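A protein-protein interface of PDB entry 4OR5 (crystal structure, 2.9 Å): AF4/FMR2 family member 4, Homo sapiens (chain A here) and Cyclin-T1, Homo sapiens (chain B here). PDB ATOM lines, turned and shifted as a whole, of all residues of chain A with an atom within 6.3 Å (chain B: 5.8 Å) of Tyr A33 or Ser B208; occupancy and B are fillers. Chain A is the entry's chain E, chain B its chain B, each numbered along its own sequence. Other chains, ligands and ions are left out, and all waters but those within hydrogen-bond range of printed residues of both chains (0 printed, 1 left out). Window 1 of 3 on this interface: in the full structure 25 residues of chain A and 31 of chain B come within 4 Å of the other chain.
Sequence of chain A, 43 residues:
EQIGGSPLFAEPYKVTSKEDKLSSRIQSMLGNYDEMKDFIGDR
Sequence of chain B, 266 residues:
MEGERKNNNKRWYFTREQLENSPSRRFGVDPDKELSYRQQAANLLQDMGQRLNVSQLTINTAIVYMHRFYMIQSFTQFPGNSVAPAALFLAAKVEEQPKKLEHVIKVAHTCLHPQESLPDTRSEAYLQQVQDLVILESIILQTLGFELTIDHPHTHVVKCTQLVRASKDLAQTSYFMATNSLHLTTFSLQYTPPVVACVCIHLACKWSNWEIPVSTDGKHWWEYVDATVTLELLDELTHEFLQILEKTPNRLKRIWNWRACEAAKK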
ATOM      1  N   LYS A  14      10.740 -12.418 -23.245  1.00  0.00           N
ATOM      2  CA  LYS A  14      11.748 -11.744 -24.057  1.00  0.00           C
ATOM      3  C   LYS A  14      11.592 -11.932 -25.558  1.00  0.00           C
ATOM      4  O   LYS A  14      11.480 -13.044 -26.058  1.00  0.00           O
ATOM      5  CB  LYS A  14      13.153 -12.165 -23.632  1.00  0.00           C
ATOM      6  CG  LYS A  14      13.575 -11.579 -22.299  1.00  0.00           C
ATOM      7  CD  LYS A  14      14.498 -10.387 -22.473  1.00  0.00           C
ATOM      8  CE  LYS A  14      14.996  -9.887 -21.119  1.00  0.00           C
ATOM      9  NZ  LYS A  14      16.274  -9.125 -21.245  1.00  0.00           N
ATOM     10  N   VAL A  15      11.574 -10.808 -26.261  1.00  0.00           N
ATOM     11  CA  VAL A  15      11.450 -10.768 -27.709  1.00  0.00           C
ATOM     12  C   VAL A  15      12.693 -10.048 -28.186  1.00  0.00           C
ATOM     13  O   VAL A  15      12.667  -8.858 -28.474  1.00  0.00           O
ATOM     14  CB  VAL A  15      10.170 -10.001 -28.139  1.00  0.00           C
ATOM     15  CG1 VAL A  15      10.276  -9.527 -29.581  1.00  0.00           C
ATOM     16  CG2 VAL A  15       8.978 -10.925 -28.008  1.00  0.00           C
ATOM     17  N   GLN A  27      18.158   1.922 -26.856  1.00  0.00           N
ATOM     18  CA  GLN A  27      19.315   1.148 -26.433  1.00  0.00           C
ATOM     19  C   GLN A  27      20.597   1.948 -26.574  1.00  0.00           C
ATOM     20  O   GLN A  27      21.396   2.010 -25.640  1.00  0.00           O
ATOM     21  CB  GLN A  27      19.427  -0.145 -27.246  1.00  0.00           C
ATOM     22  CG  GLN A  27      18.678  -1.337 -26.648  1.00  0.00           C
ATOM     23  CD  GLN A  27      18.723  -2.570 -27.544  1.00  0.00           C
ATOM     24  OE1 GLN A  27      19.782  -2.928 -28.076  1.00  0.00           O
ATOM     25  NE2 GLN A  27      17.569  -3.232 -27.709  1.00  0.00           N
ATOM     26  N   GLY A  31      22.177   2.184 -23.127  1.00  0.00           N
ATOM     27  CA  GLY A  31      23.060   1.035 -23.088  1.00  0.00           C
ATOM     28  C   GLY A  31      22.264  -0.246 -23.017  1.00  0.00           C
ATOM     29  O   GLY A  31      21.036  -0.203 -23.098  1.00  0.00           O
ATOM     30  N   ASN A  32      22.949  -1.378 -22.868  1.00  0.00           N
ATOM     31  CA  ASN A  32      22.276  -2.669 -22.782  1.00  0.00           C
ATOM     32  C   ASN A  32      21.530  -2.735 -21.458  1.00  0.00           C
ATOM     33  O   ASN A  32      22.111  -2.478 -20.397  1.00  0.00           O
ATOM     34  CB  ASN A  32      23.297  -3.801 -22.866  1.00  0.00           C
ATOM     35  CG  ASN A  32      22.646  -5.167 -22.932  1.00  0.00           C
ATOM     36  OD1 ASN A  32      22.039  -5.632 -21.963  1.00  0.00           O
ATOM     37  ND2 ASN A  32      22.763  -5.816 -24.082  1.00  0.00           N
ATOM     38  N   TYR A  33      20.244  -3.077 -21.520  1.00  0.00           N
ATOM     39  CA  TYR A  33      19.412  -3.133 -20.319  1.00  0.00           C
ATOM     40  C   TYR A  33      19.883  -4.133 -19.251  1.00  0.00           C
ATOM     41  O   TYR A  33      19.996  -3.781 -18.072  1.00  0.00           O
ATOM     42  CB  TYR A  33      17.943  -3.409 -20.702  1.00  0.00           C
ATOM     43  CG  TYR A  33      17.038  -3.650 -19.508  1.00  0.00           C
ATOM     44  CD1 TYR A  33      16.826  -2.658 -18.552  1.00  0.00           C
ATOM     45  CD2 TYR A  33      16.426  -4.882 -19.313  1.00  0.00           C
ATOM     46  CE1 TYR A  33      16.026  -2.890 -17.427  1.00  0.00           C
ATOM     47  CE2 TYR A  33      15.621  -5.124 -18.198  1.00  0.00           C
ATOM     48  CZ  TYR A  33      15.419  -4.128 -17.256  1.00  0.00           C
ATOM     49  OH  TYR A  33      14.586  -4.367 -16.165  1.00  0.00           O
ATOM     50  N   ASP A  34      20.165  -5.368 -19.660  1.00  0.00           N
ATOM     51  CA  ASP A  34      20.601  -6.402 -18.722  1.00  0.00           C
ATOM     52  C   ASP A  34      21.870  -6.029 -17.936  1.00  0.00           C
ATOM     53  O   ASP A  34      22.058  -6.453 -16.791  1.00  0.00           O
ATOM     54  CB  ASP A  34      20.761  -7.719 -19.481  1.00  0.00           C
ATOM     55  CG  ASP A  34      19.449  -8.163 -20.151  1.00  0.00           C
ATOM     56  OD1 ASP A  34      18.439  -8.379 -19.428  1.00  0.00           O
ATOM     57  OD2 ASP A  34      19.422  -8.290 -21.401  1.00  0.00           O
ATOM     58  N   GLU A  35      22.709  -5.197 -18.541  1.00  0.00           N
ATOM     59  CA  GLU A  35      23.940  -4.728 -17.915  1.00  0.00           C
ATOM     60  C   GLU A  35      23.702  -3.636 -16.879  1.00  0.00           C
ATOM     61  O   GLU A  35      24.127  -3.744 -15.728  1.00  0.00           O
ATOM     62  CB  GLU A  35      24.878  -4.172 -18.975  1.00  0.00           C
ATOM     63  CG  GLU A  35      25.259  -5.170 -20.043  1.00  0.00           C
ATOM     64  CD  GLU A  35      26.199  -4.576 -21.082  1.00  0.00           C
ATOM     65  OE1 GLU A  35      27.042  -3.715 -20.710  1.00  0.00           O
ATOM     66  OE2 GLU A  35      26.098  -4.987 -22.264  1.00  0.00           O
ATOM     67  N   MET A  36      23.015  -2.581 -17.307  1.00  0.00           N
ATOM     68  CA  MET A  36      22.712  -1.420 -16.465  1.00  0.00           C
ATOM     69  C   MET A  36      21.686  -1.718 -15.380  1.00  0.00           C
ATOM     70  O   MET A  36      21.879  -1.392 -14.202  1.00  0.00           O
ATOM     71  CB  MET A  36      22.183  -0.297 -17.344  1.00  0.00           C
ATOM     72  CG  MET A  36      23.017  -0.048 -18.580  1.00  0.00           C
ATOM     73  SD  MET A  36      24.715   0.413 -18.182  1.00  0.00           S
ATOM     74  CE  MET A  36      25.532   0.102 -19.854  1.00  0.00           C
ATOM     75  N   LYS A  37      20.590  -2.325 -15.815  1.00  0.00           N
ATOM     76  CA  LYS A  37      19.473  -2.695 -14.971  1.00  0.00           C
ATOM     77  C   LYS A  37      19.716  -2.792 -13.459  1.00  0.00           C
ATOM     78  O   LYS A  37      18.940  -2.264 -12.670  1.00  0.00           O
ATOM     79  CB  LYS A  37      18.899  -4.000 -15.517  1.00  0.00           C
ATOM     80  CG  LYS A  37      18.323  -4.928 -14.489  1.00  0.00           C
ATOM     81  CD  LYS A  37      17.821  -6.201 -15.146  1.00  0.00           C
ATOM     82  CE  LYS A  37      18.882  -6.929 -15.953  1.00  0.00           C
ATOM     83  NZ  LYS A  37      18.277  -8.089 -16.674  1.00  0.00           N
ATOM     84  N   ASP A  38      20.794  -3.441 -13.044  1.00  0.00           N
ATOM     85  CA  ASP A  38      21.047  -3.612 -11.620  1.00  0.00           C
ATOM     86  C   ASP A  38      21.592  -2.418 -10.879  1.00  0.00           C
ATOM     87  O   ASP A  38      21.651  -2.429  -9.652  1.00  0.00           O
ATOM     88  CB  ASP A  38      21.958  -4.810 -11.411  1.00  0.00           C
ATOM     89  CG  ASP A  38      21.291  -6.107 -11.813  1.00  0.00           C
ATOM     90  OD1 ASP A  38      20.757  -6.801 -10.919  1.00  0.00           O
ATOM     91  OD2 ASP A  38      21.282  -6.409 -13.029  1.00  0.00           O
ATOM     92  N   ILE A  40      20.305   0.712 -11.446  1.00  0.00           N
ATOM     93  CA  ILE A  40      19.154   1.568 -11.251  1.00  0.00           C
ATOM     94  C   ILE A  40      18.576   1.487  -9.853  1.00  0.00           C
ATOM     95  O   ILE A  40      18.022   0.471  -9.457  1.00  0.00           O
ATOM     96  CB  ILE A  40      18.062   1.216 -12.244  1.00  0.00           C
ATOM     97  CG1 ILE A  40      18.677   1.066 -13.635  1.00  0.00           C
ATOM     98  CG2 ILE A  40      16.985   2.287 -12.226  1.00  0.00           C
ATOM     99  CD1 ILE A  40      17.729   0.505 -14.672  1.00  0.00           C
ATOM    100  N   SER B 167       8.328  -7.951 -14.394  1.00  0.00           N
ATOM    101  CA  SER B 167       9.514  -8.262 -13.604  1.00  0.00           C
ATOM    102  C   SER B 167       9.763  -7.199 -12.535  1.00  0.00           C
ATOM    103  O   SER B 167       9.177  -6.128 -12.564  1.00  0.00           O
ATOM    104  CB  SER B 167      10.739  -8.321 -14.508  1.00  0.00           C
ATOM    105  OG  SER B 167      11.886  -7.968 -13.757  1.00  0.00           O
ATOM    106  N   ASP B 169      12.734  -5.469 -11.848  1.00  0.00           N
ATOM    107  CA  ASP B 169      13.405  -4.322 -12.425  1.00  0.00           C
ATOM    108  C   ASP B 169      12.675  -3.737 -13.614  1.00  0.00           C
ATOM    109  O   ASP B 169      12.837  -2.555 -13.912  1.00  0.00           O
ATOM    110  CB  ASP B 169      14.860  -4.645 -12.777  1.00  0.00           C
ATOM    111  CG  ASP B 169      15.694  -4.936 -11.541  1.00  0.00           C
ATOM    112  OD1 ASP B 169      15.791  -6.129 -11.200  1.00  0.00           O
ATOM    113  OD2 ASP B 169      16.228  -3.994 -10.906  1.00  0.00           O
ATOM    114  N   LEU B 170      11.865  -4.529 -14.301  1.00  0.00           N
ATOM    115  CA  LEU B 170      11.122  -3.946 -15.411  1.00  0.00           C
ATOM    116  C   LEU B 170      10.173  -2.940 -14.794  1.00  0.00           C
ATOM    117  O   LEU B 170      10.019  -1.835 -15.289  1.00  0.00           O
ATOM    118  CB  LEU B 170      10.293  -4.980 -16.158  1.00  0.00           C
ATOM    119  CG  LEU B 170       9.358  -4.329 -17.182  1.00  0.00           C
ATOM    120  CD1 LEU B 170      10.168  -3.582 -18.209  1.00  0.00           C
ATOM    121  CD2 LEU B 170       8.534  -5.378 -17.876  1.00  0.00           C
ATOM    122  N   ALA B 171       9.543  -3.336 -13.697  1.00  0.00           N
ATOM    123  CA  ALA B 171       8.605  -2.469 -13.003  1.00  0.00           C
ATOM    124  C   ALA B 171       9.323  -1.248 -12.471  1.00  0.00           C
ATOM    125  O   ALA B 171       8.744  -0.164 -12.375  1.00  0.00           O
ATOM    126  CB  ALA B 171       7.951  -3.215 -11.867  1.00  0.00           C
ATOM    127  N   THR B 173      12.276   0.007 -13.862  1.00  0.00           N
ATOM    128  CA  THR B 173      12.626   0.826 -15.009  1.00  0.00           C
ATOM    129  C   THR B 173      11.416   1.672 -15.394  1.00  0.00           C
ATOM    130  O   THR B 173      11.559   2.846 -15.699  1.00  0.00           O
ATOM    131  CB  THR B 173      13.040  -0.042 -16.212  1.00  0.00           C
ATOM    132  OG1 THR B 173      14.344  -0.579 -15.977  1.00  0.00           O
ATOM    133  CG2 THR B 173      13.063   0.779 -17.494  1.00  0.00           C
ATOM    134  N   LEU B 203       7.868   2.151 -23.212  1.00  0.00           N
ATOM    135  CA  LEU B 203       9.268   2.504 -23.396  1.00  0.00           C
ATOM    136  C   LEU B 203      10.245   1.498 -22.776  1.00  0.00           C
ATOM    137  O   LEU B 203      11.194   1.049 -23.433  1.00  0.00           O
ATOM    138  CB  LEU B 203       9.496   3.916 -22.840  1.00  0.00           C
ATOM    139  CG  LEU B 203      10.776   4.677 -23.215  1.00  0.00           C
ATOM    140  CD1 LEU B 203      11.190   4.366 -24.660  1.00  0.00           C
ATOM    141  CD2 LEU B 203      10.542   6.183 -23.000  1.00  0.00           C
ATOM    142  N   ALA B 204      10.000   1.151 -21.514  1.00  0.00           N
ATOM    143  CA  ALA B 204      10.825   0.201 -20.783  1.00  0.00           C
ATOM    144  C   ALA B 204      10.839  -1.144 -21.507  1.00  0.00           C
ATOM    145  O   ALA B 204      11.897  -1.714 -21.758  1.00  0.00           O
ATOM    146  CB  ALA B 204      10.287   0.034 -19.371  1.00  0.00           C
ATOM    147  N   CYS B 205       9.667  -1.653 -21.854  1.00  0.00           N
ATOM    148  CA  CYS B 205       9.609  -2.923 -22.546  1.00  0.00           C
ATOM    149  C   CYS B 205      10.441  -2.882 -23.820  1.00  0.00           C
ATOM    150  O   CYS B 205      10.936  -3.907 -24.281  1.00  0.00           O
ATOM    151  CB  CYS B 205       8.159  -3.269 -22.873  1.00  0.00           C
ATOM    152  SG  CYS B 205       7.207  -3.427 -21.386  1.00  0.00           S
ATOM    153  N   LYS B 206      10.603  -1.697 -24.386  1.00  0.00           N
ATOM    154  CA  LYS B 206      11.354  -1.569 -25.618  1.00  0.00           C
ATOM    155  C   LYS B 206      12.841  -1.653 -25.337  1.00  0.00           C
ATOM    156  O   LYS B 206      13.630  -2.133 -26.161  1.00  0.00           O
ATOM    157  CB  LYS B 206      11.015  -0.245 -26.291  1.00  0.00           C
ATOM    158  CG  LYS B 206       9.621  -0.207 -26.893  1.00  0.00           C
ATOM    159  CD  LYS B 206       9.563  -1.103 -28.098  1.00  0.00           C
ATOM    160  CE  LYS B 206       8.151  -1.286 -28.580  1.00  0.00           C
ATOM    161  NZ  LYS B 206       8.183  -2.246 -29.718  1.00  0.00           N
ATOM    162  N   TRP B 207      13.221  -1.190 -24.155  1.00  0.00           N
ATOM    163  CA  TRP B 207      14.614  -1.206 -23.755  1.00  0.00           C
ATOM    164  C   TRP B 207      15.030  -2.604 -23.260  1.00  0.00           C
ATOM    165  O   TRP B 207      16.181  -3.024 -23.441  1.00  0.00           O
ATOM    166  CB  TRP B 207      14.818  -0.151 -22.662  1.00  0.00           C
ATOM    167  CG  TRP B 207      16.243   0.006 -22.181  1.00  0.00           C
ATOM    168  CD1 TRP B 207      17.390  -0.180 -22.914  1.00  0.00           C
ATOM    169  CD2 TRP B 207      16.674   0.465 -20.890  1.00  0.00           C
ATOM    170  NE1 TRP B 207      18.499   0.139 -22.159  1.00  0.00           N
ATOM    171  CE2 TRP B 207      18.087   0.541 -20.918  1.00  0.00           C
ATOM    172  CE3 TRP B 207      16.002   0.825 -19.716  1.00  0.00           C
ATOM    173  CZ2 TRP B 207      18.833   0.959 -19.823  1.00  0.00           C
ATOM    174  CZ3 TRP B 207      16.753   1.241 -18.619  1.00  0.00           C
ATOM    175  CH2 TRP B 207      18.155   1.307 -18.686  1.00  0.00           C
ATOM    176  N   SER B 208      14.075  -3.322 -22.669  1.00  0.00           N
ATOM    177  CA  SER B 208      14.299  -4.648 -22.101  1.00  0.00           C
ATOM    178  C   SER B 208      13.737  -5.827 -22.890  1.00  0.00           C
ATOM    179  O   SER B 208      13.703  -6.948 -22.395  1.00  0.00           O
ATOM    180  CB  SER B 208      13.699  -4.675 -20.706  1.00  0.00           C
ATOM    181  OG  SER B 208      12.373  -4.189 -20.743  1.00  0.00           O
ATOM    182  N   ASN B 209      13.287  -5.581 -24.109  1.00  0.00           N
ATOM    183  CA  ASN B 209      12.719  -6.642 -24.923  1.00  0.00           C
ATOM    184  C   ASN B 209      11.596  -7.426 -24.253  1.00  0.00           C
ATOM    185  O   ASN B 209      11.357  -8.569 -24.602  1.00  0.00           O
ATOM    186  CB  ASN B 209      13.815  -7.593 -25.343  1.00  0.00           C
ATOM    187  CG  ASN B 209      14.922  -6.887 -26.045  1.00  0.00           C
ATOM    188  OD1 ASN B 209      14.710  -6.231 -27.073  1.00  0.00           O
ATOM    189  ND2 ASN B 209      16.121  -7.000 -25.501  1.00  0.00           N
ATOM    190  N   TRP B 210      10.904  -6.817 -23.298  1.00  0.00           N
ATOM    191  CA  TRP B 210       9.809  -7.500 -22.631  1.00  0.00           C
ATOM    192  C   TRP B 210       8.533  -7.302 -23.420  1.00  0.00           C
ATOM    193  O   TRP B 210       8.183  -6.176 -23.777  1.00  0.00           O
ATOM    194  CB  TRP B 210       9.626  -6.968 -21.209  1.00  0.00           C
ATOM    195  CG  TRP B 210      10.578  -7.566 -20.207  1.00  0.00           C
ATOM    196  CD1 TRP B 210      11.344  -6.891 -19.301  1.00  0.00           C
ATOM    197  CD2 TRP B 210      10.859  -8.962 -20.007  1.00  0.00           C
ATOM    198  NE1 TRP B 210      12.085  -7.774 -18.553  1.00  0.00           N
ATOM    199  CE2 TRP B 210      11.807  -9.050 -18.965  1.00  0.00           C
ATOM    200  CE3 TRP B 210      10.399 -10.146 -20.607  1.00  0.00           C
ATOM    201  CZ2 TRP B 210      12.309 -10.272 -18.511  1.00  0.00           C
ATOM    202  CZ3 TRP B 210      10.899 -11.357 -20.153  1.00  0.00           C
ATOM    203  CH2 TRP B 210      11.845 -11.408 -19.113  1.00  0.00           C
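The indole nitrogen (NE1) of Trp B207 is in hydrogen-bond range of the backbone carbonyl oxygen (O) of Gly A31, 2.7 Å away.
N of Leu B170 is in hydrogen-bond range of OH of Tyr A33, at 3.3 Å.
O of Asn B209 is in hydrogen-bond range of N of Val A15 (2.8 Å).
The side-chain hydroxyl (OH) of Tyr A33 sits close to the backbone carbonyl oxygen (O) of Asp B169 (3.4 Å).
The side-chain carboxylate (OD1) of Asp A34 is in salt-bridge range of the side-chain amino group (NZ) of Lys A37.
O of Cys B205 lies within hydrogen-bond range of N of Trp B210 (3.1 Å).
The backbone NH (N) of Asp B169 sits at hydrogen-bond distance from the side-chain hydroxyl (OG) of Ser B167 (3.3 Å).
The side-chain hydroxyl (OG) of Ser B167 sits at hydrogen-bond distance from the backbone NH (N) of Leu B170, at 3.5 Å.
OG of Ser B208 sits at hydrogen-bond distance from O of Ala B204.
O of Asp B169 lies within hydrogen-bond range of OG1 of Thr B173 (3.2 Å).
Among the printed residues, merely in contact across the chains: Tyr A33 with Ser B208 (3.1 Å), Tyr A33 with Thr B173 (3.2 Å), Lys A14 with Asn B209 (3.2 Å), Lys A14 with Trp B210 (3.3 Å), Tyr A33 with Trp B207 (3.3 Å), Lys A14 with Ser B208 (3.5 Å), Lys A37 with Asp B169 (3.7 Å) and Ile A40 with Thr B173 (3.8 Å).
Printed residues of chain B within 4 Å of Gly A31: Trp B207 (2.7 Å).
Of chain B, only Asp B169 (3.2 Å), Leu B170 (3.3 Å), Thr B173 (3.2 Å), Trp B207 (3.3 Å) and Ser B208 (3.1 Å) come within 4 Å of Tyr A33.
Asp A38 touches none of the printed residues of chain B.
Printed residues of chain A within 4 Å of Asp B169: Tyr A33 (3.2 Å) and Lys A37 (3.7 Å).
The nearest printed residue of chain B that does not touch Lys A37 is Trp B207 (5.2 Å).
Of the 12 printed residues of chain A, 6 touch a printed residue of chain B.
Hydrophobic or aromatic side chains of chain B that line the printed part of chain A: Trp B207 and Trp B210.
Among the printed residues, 12 pairs touch across the chains.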
